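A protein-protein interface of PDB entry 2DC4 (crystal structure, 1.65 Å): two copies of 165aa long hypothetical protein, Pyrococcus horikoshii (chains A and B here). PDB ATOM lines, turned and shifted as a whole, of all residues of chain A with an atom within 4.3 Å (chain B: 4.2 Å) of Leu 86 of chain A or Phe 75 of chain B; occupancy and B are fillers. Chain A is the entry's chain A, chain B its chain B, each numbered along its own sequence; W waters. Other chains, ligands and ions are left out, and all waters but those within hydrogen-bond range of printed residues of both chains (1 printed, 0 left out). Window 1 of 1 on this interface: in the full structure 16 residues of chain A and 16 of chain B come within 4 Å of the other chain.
The side-chain carboxylate (OD1) of Asp 79 of chain A is in hydrogen-bond range of the backbone NH (N) of Gly 82 of chain A. The backbone NH (N) of Ile 57 of chain B is in hydrogen-bond range of the backbone carbonyl oxygen (O) of Phe 75 of chain B (3.0 Å). The side-chain carboxylate (OE2) of Glu 85 of chain A lies within salt-bridge range of the guanidinium group (NE) of Arg 89 of chain A (2.9 Å). O of Leu 73 of chain B lies within hydrogen-bond range of N of Tyr 59 of chain B, 2.8 Å away.
Among the printed residues, merely in contact across the chains: Val 77 of chain A with Glu 76 of chain B (3.6 Å), Val 77 of chain A with Val 77 of chain B (3.8 Å), Asp 79 of chain A with Phe 75 of chain B (3.5 Å), Gly 82 of chain A with Leu 73 of chain B (3.6 Å), Gly 82 of chain A with Phe 75 of chain B (3.8 Å), Ala 83 of chain A with Phe 75 of chain B (3.8 Å), Glu 85 of chain A with Leu 73 of chain B (3.5 Å), Leu 86 of chain A with Ile 57 of chain B (3.6 Å), Leu 86 of chain A with Tyr 59 of chain B (3.6 Å), Leu 86 of chain A with Leu 73 of chain B (3.6 Å), Leu 86 of chain A with Phe 75 of chain B (3.996 Å) and Arg 89 of chain A with Tyr 59 of chain B (3.8 Å).
Of the printed residues of chain B, Leu 86 of chain A touches Ile 57, Tyr 59, Leu 73 and Phe 75. Printed residues of chain B within 4 Å of Glu 85 of chain A: Leu 73. Of the printed residues of chain A, Val 77 of chain B touches Val 77. Ile 84 of chain A touches none of the printed residues of chain B. The nearest printed residue of chain B that does not touch Leu 86 of chain A is Phe 87 of chain B (4.1 Å). The nearest printed residue of chain A that does not touch Val 77 of chain B is Asp 79 of chain A (6.9 Å).
Of the 11 printed residues of chain A, 7 touch a printed residue of chain B. Printed residues of chain A that touch a printed residue of chain B: Val 77, Asp 79, Gly 82, Ala 83, Glu 85, Leu 86 and Arg 89. Among the printed residues, 12 pairs touch across the chains. Among the printed residues, no Asp or Glu carboxylate lies within 4 Å of a Lys or Arg side-chain nitrogen of the other chain.
Val 77 of chain A touches its own counterpart, Val 77 of chain B. 2 positions are printed for both chains. Of the 12 pairs that touch across the chains among the printed residues, 1 has its exchanged pair printed and touching as well.
Water W1 bridges OD2 of Asp 79 of chain A and O of Glu 74 of chain B.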
ATOM      1  N   VAL A  77     -22.137  20.644 -18.325  1.00  0.00           N
ATOM      2  CA  VAL A  77     -21.110  21.529 -18.875  1.00  0.00           C
ATOM      3  C   VAL A  77     -20.207  20.671 -19.747  1.00  0.00           C
ATOM      4  O   VAL A  77     -20.125  19.457 -19.560  1.00  0.00           O
ATOM      5  CB  VAL A  77     -20.266  22.237 -17.781  1.00  0.00           C
ATOM      6  CG1 VAL A  77     -21.189  23.049 -16.870  1.00  0.00           C
ATOM      7  CG2 VAL A  77     -19.447  21.227 -16.983  1.00  0.00           C
ATOM      8  N   ASP A  79     -16.862  21.215 -20.133  1.00  0.00           N
ATOM      9  CA  ASP A  79     -15.477  21.232 -19.665  1.00  0.00           C
ATOM     10  C   ASP A  79     -15.403  21.258 -18.145  1.00  0.00           C
ATOM     11  O   ASP A  79     -15.443  22.320 -17.529  1.00  0.00           O
ATOM     12  CB  ASP A  79     -14.763  22.453 -20.262  1.00  0.00           C
ATOM     13  CG  ASP A  79     -13.341  22.610 -19.757  1.00  0.00           C
ATOM     14  OD1 ASP A  79     -12.800  21.646 -19.175  1.00  0.00           O
ATOM     15  OD2 ASP A  79     -12.762  23.703 -19.955  1.00  0.00           O
ATOM     16  N   GLY A  82     -12.365  23.090 -16.789  1.00  0.00           N
ATOM     17  CA  GLY A  82     -12.560  24.526 -16.863  1.00  0.00           C
ATOM     18  C   GLY A  82     -13.475  25.024 -15.762  1.00  0.00           C
ATOM     19  O   GLY A  82     -13.268  26.097 -15.212  1.00  0.00           O
ATOM     20  N   ALA A  83     -14.497  24.240 -15.435  1.00  0.00           N
ATOM     21  CA  ALA A  83     -15.428  24.633 -14.381  1.00  0.00           C
ATOM     22  C   ALA A  83     -14.722  24.670 -13.027  1.00  0.00           C
ATOM     23  O   ALA A  83     -14.977  25.549 -12.197  1.00  0.00           O
ATOM     24  CB  ALA A  83     -16.600  23.662 -14.336  1.00  0.00           C
ATOM     25  N   ILE A  84     -13.839  23.705 -12.798  1.00  0.00           N
ATOM     26  CA  ILE A  84     -13.094  23.655 -11.547  1.00  0.00           C
ATOM     27  C   ILE A  84     -12.142  24.850 -11.482  1.00  0.00           C
ATOM     28  O   ILE A  84     -12.029  25.509 -10.447  1.00  0.00           O
ATOM     29  CB  ILE A  84     -12.331  22.319 -11.433  1.00  0.00           C
ATOM     30  CG1 ILE A  84     -13.344  21.201 -11.152  1.00  0.00           C
ATOM     31  CG2 ILE A  84     -11.279  22.399 -10.325  1.00  0.00           C
ATOM     32  CD1 ILE A  84     -12.818  19.793 -11.354  1.00  0.00           C
ATOM     33  N   GLU A  85     -11.481  25.145 -12.596  1.00  0.00           N
ATOM     34  CA  GLU A  85     -10.566  26.283 -12.648  1.00  0.00           C
ATOM     35  C   GLU A  85     -11.336  27.574 -12.368  1.00  0.00           C
ATOM     36  O   GLU A  85     -10.881  28.433 -11.612  1.00  0.00           O
ATOM     37  CB  GLU A  85      -9.906  26.375 -14.025  1.00  0.00           C
ATOM     38  CG  GLU A  85      -8.884  27.494 -14.130  1.00  0.00           C
ATOM     39  CD  GLU A  85      -8.403  27.715 -15.542  1.00  0.00           C
ATOM     40  OE1 GLU A  85      -8.192  26.722 -16.269  1.00  0.00           O
ATOM     41  OE2 GLU A  85      -8.223  28.891 -15.922  1.00  0.00           O
ATOM     42  N   LEU A  86     -12.506  27.707 -12.984  1.00  0.00           N
ATOM     43  CA  LEU A  86     -13.336  28.889 -12.793  1.00  0.00           C
ATOM     44  C   LEU A  86     -13.664  29.170 -11.332  1.00  0.00           C
ATOM     45  O   LEU A  86     -13.481  30.288 -10.857  1.00  0.00           O
ATOM     46  CB  LEU A  86     -14.646  28.749 -13.572  1.00  0.00           C
ATOM     47  CG  LEU A  86     -15.693  29.839 -13.322  1.00  0.00           C
ATOM     48  CD1 LEU A  86     -15.180  31.164 -13.859  1.00  0.00           C
ATOM     49  CD2 LEU A  86     -17.002  29.466 -14.009  1.00  0.00           C
ATOM     50  N   PHE A  87     -14.158  28.170 -10.611  1.00  0.00           N
ATOM     51  CA  PHE A  87     -14.506  28.412  -9.220  1.00  0.00           C
ATOM     52  C   PHE A  87     -13.294  28.763  -8.371  1.00  0.00           C
ATOM     53  O   PHE A  87     -13.395  29.568  -7.447  1.00  0.00           O
ATOM     54  CB  PHE A  87     -15.284  27.219  -8.662  1.00  0.00           C
ATOM     55  CG  PHE A  87     -16.651  27.084  -9.264  1.00  0.00           C
ATOM     56  CD1 PHE A  87     -17.537  28.159  -9.228  1.00  0.00           C
ATOM     57  CD2 PHE A  87     -17.047  25.910  -9.909  1.00  0.00           C
ATOM     58  CE1 PHE A  87     -18.789  28.075  -9.821  1.00  0.00           C
ATOM     59  CE2 PHE A  87     -18.302  25.818 -10.506  1.00  0.00           C
ATOM     60  CZ  PHE A  87     -19.173  26.903 -10.461  1.00  0.00           C
ATOM     61  N   LYS A  88     -12.145  28.185  -8.697  1.00  0.00           N
ATOM     62  CA  LYS A  88     -10.932  28.513  -7.960  1.00  0.00           C
ATOM     63  C   LYS A  88     -10.572  29.971  -8.238  1.00  0.00           C
ATOM     64  O   LYS A  88     -10.223  30.714  -7.324  1.00  0.00           O
ATOM     65  CB  LYS A  88      -9.769  27.621  -8.389  1.00  0.00           C
ATOM     66  CG  LYS A  88      -9.862  26.183  -7.913  1.00  0.00           C
ATOM     67  CD  LYS A  88      -8.658  25.397  -8.406  1.00  0.00           C
ATOM     68  CE  LYS A  88      -8.695  23.955  -7.952  1.00  0.00           C
ATOM     69  NZ  LYS A  88      -7.542  23.201  -8.525  1.00  0.00           N
ATOM     70  N   ARG A  89     -10.657  30.381  -9.501  1.00  0.00           N
ATOM     71  CA  ARG A  89     -10.327  31.760  -9.856  1.00  0.00           C
ATOM     72  C   ARG A  89     -11.325  32.769  -9.299  1.00  0.00           C
ATOM     73  O   ARG A  89     -11.009  33.952  -9.169  1.00  0.00           O
ATOM     74  CB  ARG A  89     -10.205  31.910 -11.374  1.00  0.00           C
ATOM     75  CG  ARG A  89      -8.969  31.211 -11.931  1.00  0.00           C
ATOM     76  CD  ARG A  89      -8.705  31.554 -13.389  1.00  0.00           C
ATOM     77  NE  ARG A  89      -7.530  30.852 -13.900  1.00  0.00           N
ATOM     78  CZ  ARG A  89      -6.284  31.086 -13.500  1.00  0.00           C
ATOM     79  NH1 ARG A  89      -6.037  32.010 -12.581  1.00  0.00           N
ATOM     80  NH2 ARG A  89      -5.280  30.389 -14.014  1.00  0.00           N
ATOM     81  N   LEU A  90     -12.523  32.301  -8.960  1.00  0.00           N
ATOM     82  CA  LEU A  90     -13.544  33.172  -8.396  1.00  0.00           C
ATOM     83  C   LEU A  90     -13.357  33.299  -6.886  1.00  0.00           C
ATOM     84  O   LEU A  90     -14.095  34.023  -6.222  1.00  0.00           O
ATOM     85  CB  LEU A  90     -14.946  32.638  -8.712  1.00  0.00           C
ATOM     86  CG  LEU A  90     -15.371  32.731 -10.180  1.00  0.00           C
ATOM     87  CD1 LEU A  90     -16.750  32.121 -10.371  1.00  0.00           C
ATOM     88  CD2 LEU A  90     -15.371  34.197 -10.608  1.00  0.00           C
ATOM     89  N   TYR B  56     -22.531  29.731 -23.182  1.00  0.00           N
ATOM     90  CA  TYR B  56     -21.226  29.614 -22.531  1.00  0.00           C
ATOM     91  C   TYR B  56     -21.107  30.378 -21.227  1.00  0.00           C
ATOM     92  O   TYR B  56     -21.874  31.294 -20.946  1.00  0.00           O
ATOM     93  CB  TYR B  56     -20.122  30.167 -23.442  1.00  0.00           C
ATOM     94  CG  TYR B  56     -20.054  29.529 -24.796  1.00  0.00           C
ATOM     95  CD1 TYR B  56     -20.899  29.940 -25.833  1.00  0.00           C
ATOM     96  CD2 TYR B  56     -19.188  28.467 -25.031  1.00  0.00           C
ATOM     97  CE1 TYR B  56     -20.877  29.297 -27.070  1.00  0.00           C
ATOM     98  CE2 TYR B  56     -19.161  27.822 -26.257  1.00  0.00           C
ATOM     99  CZ  TYR B  56     -20.006  28.236 -27.267  1.00  0.00           C
ATOM    100  OH  TYR B  56     -19.994  27.564 -28.461  1.00  0.00           O
ATOM    101  N   ILE B  57     -20.127  29.980 -20.427  1.00  0.00           N
ATOM    102  CA  ILE B  57     -19.806  30.713 -19.213  1.00  0.00           C
ATOM    103  C   ILE B  57     -18.414  31.215 -19.585  1.00  0.00           C
ATOM    104  O   ILE B  57     -17.588  30.436 -20.079  1.00  0.00           O
ATOM    105  CB  ILE B  57     -19.696  29.824 -17.965  1.00  0.00           C
ATOM    106  CG1 ILE B  57     -21.093  29.388 -17.510  1.00  0.00           C
ATOM    107  CG2 ILE B  57     -18.971  30.595 -16.856  1.00  0.00           C
ATOM    108  CD1 ILE B  57     -21.103  28.489 -16.277  1.00  0.00           C
ATOM    109  N   TYR B  59     -15.023  33.703 -18.313  1.00  0.00           N
ATOM    110  CA  TYR B  59     -14.302  34.457 -17.294  1.00  0.00           C
ATOM    111  C   TYR B  59     -13.090  35.074 -17.970  1.00  0.00           C
ATOM    112  O   TYR B  59     -12.411  34.419 -18.764  1.00  0.00           O
ATOM    113  CB  TYR B  59     -13.845  33.536 -16.158  1.00  0.00           C
ATOM    114  CG  TYR B  59     -12.816  34.144 -15.218  1.00  0.00           C
ATOM    115  CD1 TYR B  59     -11.456  34.125 -15.532  1.00  0.00           C
ATOM    116  CD2 TYR B  59     -13.202  34.713 -14.006  1.00  0.00           C
ATOM    117  CE1 TYR B  59     -10.508  34.657 -14.659  1.00  0.00           C
ATOM    118  CE2 TYR B  59     -12.264  35.245 -13.126  1.00  0.00           C
ATOM    119  CZ  TYR B  59     -10.920  35.212 -13.459  1.00  0.00           C
ATOM    120  OH  TYR B  59      -9.994  35.735 -12.581  1.00  0.00           O
ATOM    121  N   LEU B  73     -11.130  32.203 -20.000  1.00  0.00           N
ATOM    122  CA  LEU B  73     -11.530  30.849 -19.645  1.00  0.00           C
ATOM    123  C   LEU B  73     -12.984  30.753 -20.065  1.00  0.00           C
ATOM    124  O   LEU B  73     -13.844  31.427 -19.502  1.00  0.00           O
ATOM    125  CB  LEU B  73     -11.400  30.623 -18.138  1.00  0.00           C
ATOM    126  CG  LEU B  73     -11.925  29.294 -17.584  1.00  0.00           C
ATOM    127  CD1 LEU B  73     -11.237  28.117 -18.261  1.00  0.00           C
ATOM    128  CD2 LEU B  73     -11.689  29.262 -16.085  1.00  0.00           C
ATOM    129  N   GLU B  74     -13.254  29.929 -21.065  1.00  0.00           N
ATOM    130  CA  GLU B  74     -14.612  29.789 -21.567  1.00  0.00           C
ATOM    131  C   GLU B  74     -14.979  28.350 -21.870  1.00  0.00           C
ATOM    132  O   GLU B  74     -14.184  27.591 -22.425  1.00  0.00           O
ATOM    133  CB  GLU B  74     -14.784  30.625 -22.834  1.00  0.00           C
ATOM    134  CG  GLU B  74     -16.120  30.418 -23.532  1.00  0.00           C
ATOM    135  CD  GLU B  74     -16.300  31.337 -24.712  1.00  0.00           C
ATOM    136  OE1 GLU B  74     -16.400  32.561 -24.496  1.00  0.00           O
ATOM    137  OE2 GLU B  74     -16.333  30.839 -25.858  1.00  0.00           O
ATOM    138  N   PHE B  75     -16.194  27.969 -21.504  1.00  0.00           N
ATOM    139  CA  PHE B  75     -16.648  26.623 -21.793  1.00  0.00           C
ATOM    140  C   PHE B  75     -18.144  26.618 -22.013  1.00  0.00           C
ATOM    141  O   PHE B  75     -18.871  27.458 -21.478  1.00  0.00           O
ATOM    142  CB  PHE B  75     -16.244  25.627 -20.687  1.00  0.00           C
ATOM    143  CG  PHE B  75     -16.739  25.982 -19.316  1.00  0.00           C
ATOM    144  CD1 PHE B  75     -18.003  25.577 -18.882  1.00  0.00           C
ATOM    145  CD2 PHE B  75     -15.932  26.704 -18.443  1.00  0.00           C
ATOM    146  CE1 PHE B  75     -18.446  25.885 -17.590  1.00  0.00           C
ATOM    147  CE2 PHE B  75     -16.364  27.016 -17.159  1.00  0.00           C
ATOM    148  CZ  PHE B  75     -17.624  26.605 -16.729  1.00  0.00           C
ATOM    149  N   GLU B  76     -18.587  25.677 -22.833  1.00  0.00           N
ATOM    150  CA  GLU B  76     -19.996  25.548 -23.171  1.00  0.00           C
ATOM    151  C   GLU B  76     -20.798  24.938 -22.029  1.00  0.00           C
ATOM    152  O   GLU B  76     -20.307  24.058 -21.329  1.00  0.00           O
ATOM    153  CB  GLU B  76     -20.148  24.660 -24.408  1.00  0.00           C
ATOM    154  CG  GLU B  76     -21.569  24.619 -24.963  1.00  0.00           C
ATOM    155  CD  GLU B  76     -21.725  23.659 -26.129  1.00  0.00           C
ATOM    156  OE1 GLU B  76     -20.763  23.492 -26.900  1.00  0.00           O
ATOM    157  OE2 GLU B  76     -22.820  23.082 -26.285  1.00  0.00           O
ATOM    158  N   VAL B  77     -22.024  25.424 -21.843  1.00  0.00           N
ATOM    159  CA  VAL B  77     -22.919  24.887 -20.822  1.00  0.00           C
ATOM    160  C   VAL B  77     -24.248  24.613 -21.513  1.00  0.00           C
ATOM    161  O   VAL B  77     -24.575  25.249 -22.508  1.00  0.00           O
ATOM    162  CB  VAL B  77     -23.142  25.870 -19.648  1.00  0.00           C
ATOM    163  CG1 VAL B  77     -21.805  26.189 -18.990  1.00  0.00           C
ATOM    164  CG2 VAL B  77     -23.825  27.148 -20.133  1.00  0.00           C
ATOM    165  N   PHE B  87     -24.971  31.816 -10.420  1.00  0.00           N
ATOM    166  CA  PHE B  87     -24.144  32.916  -9.962  1.00  0.00           C
ATOM    167  C   PHE B  87     -24.888  33.847  -9.021  1.00  0.00           C
ATOM    168  O   PHE B  87     -24.308  34.361  -8.070  1.00  0.00           O
ATOM    169  CB  PHE B  87     -23.543  33.645 -11.162  1.00  0.00           C
ATOM    170  CG  PHE B  87     -22.509  32.825 -11.882  1.00  0.00           C
ATOM    171  CD1 PHE B  87     -22.633  32.532 -13.242  1.00  0.00           C
ATOM    172  CD2 PHE B  87     -21.428  32.298 -11.181  1.00  0.00           C
ATOM    173  CE1 PHE B  87     -21.693  31.725 -13.880  1.00  0.00           C
ATOM    174  CE2 PHE B  87     -20.490  31.493 -11.809  1.00  0.00           C
ATOM    175  CZ  PHE B  87     -20.622  31.205 -13.158  1.00  0.00           C
HETATM  176  O   HOH W   1     -12.406  25.680 -21.627  1.00  0.00           O
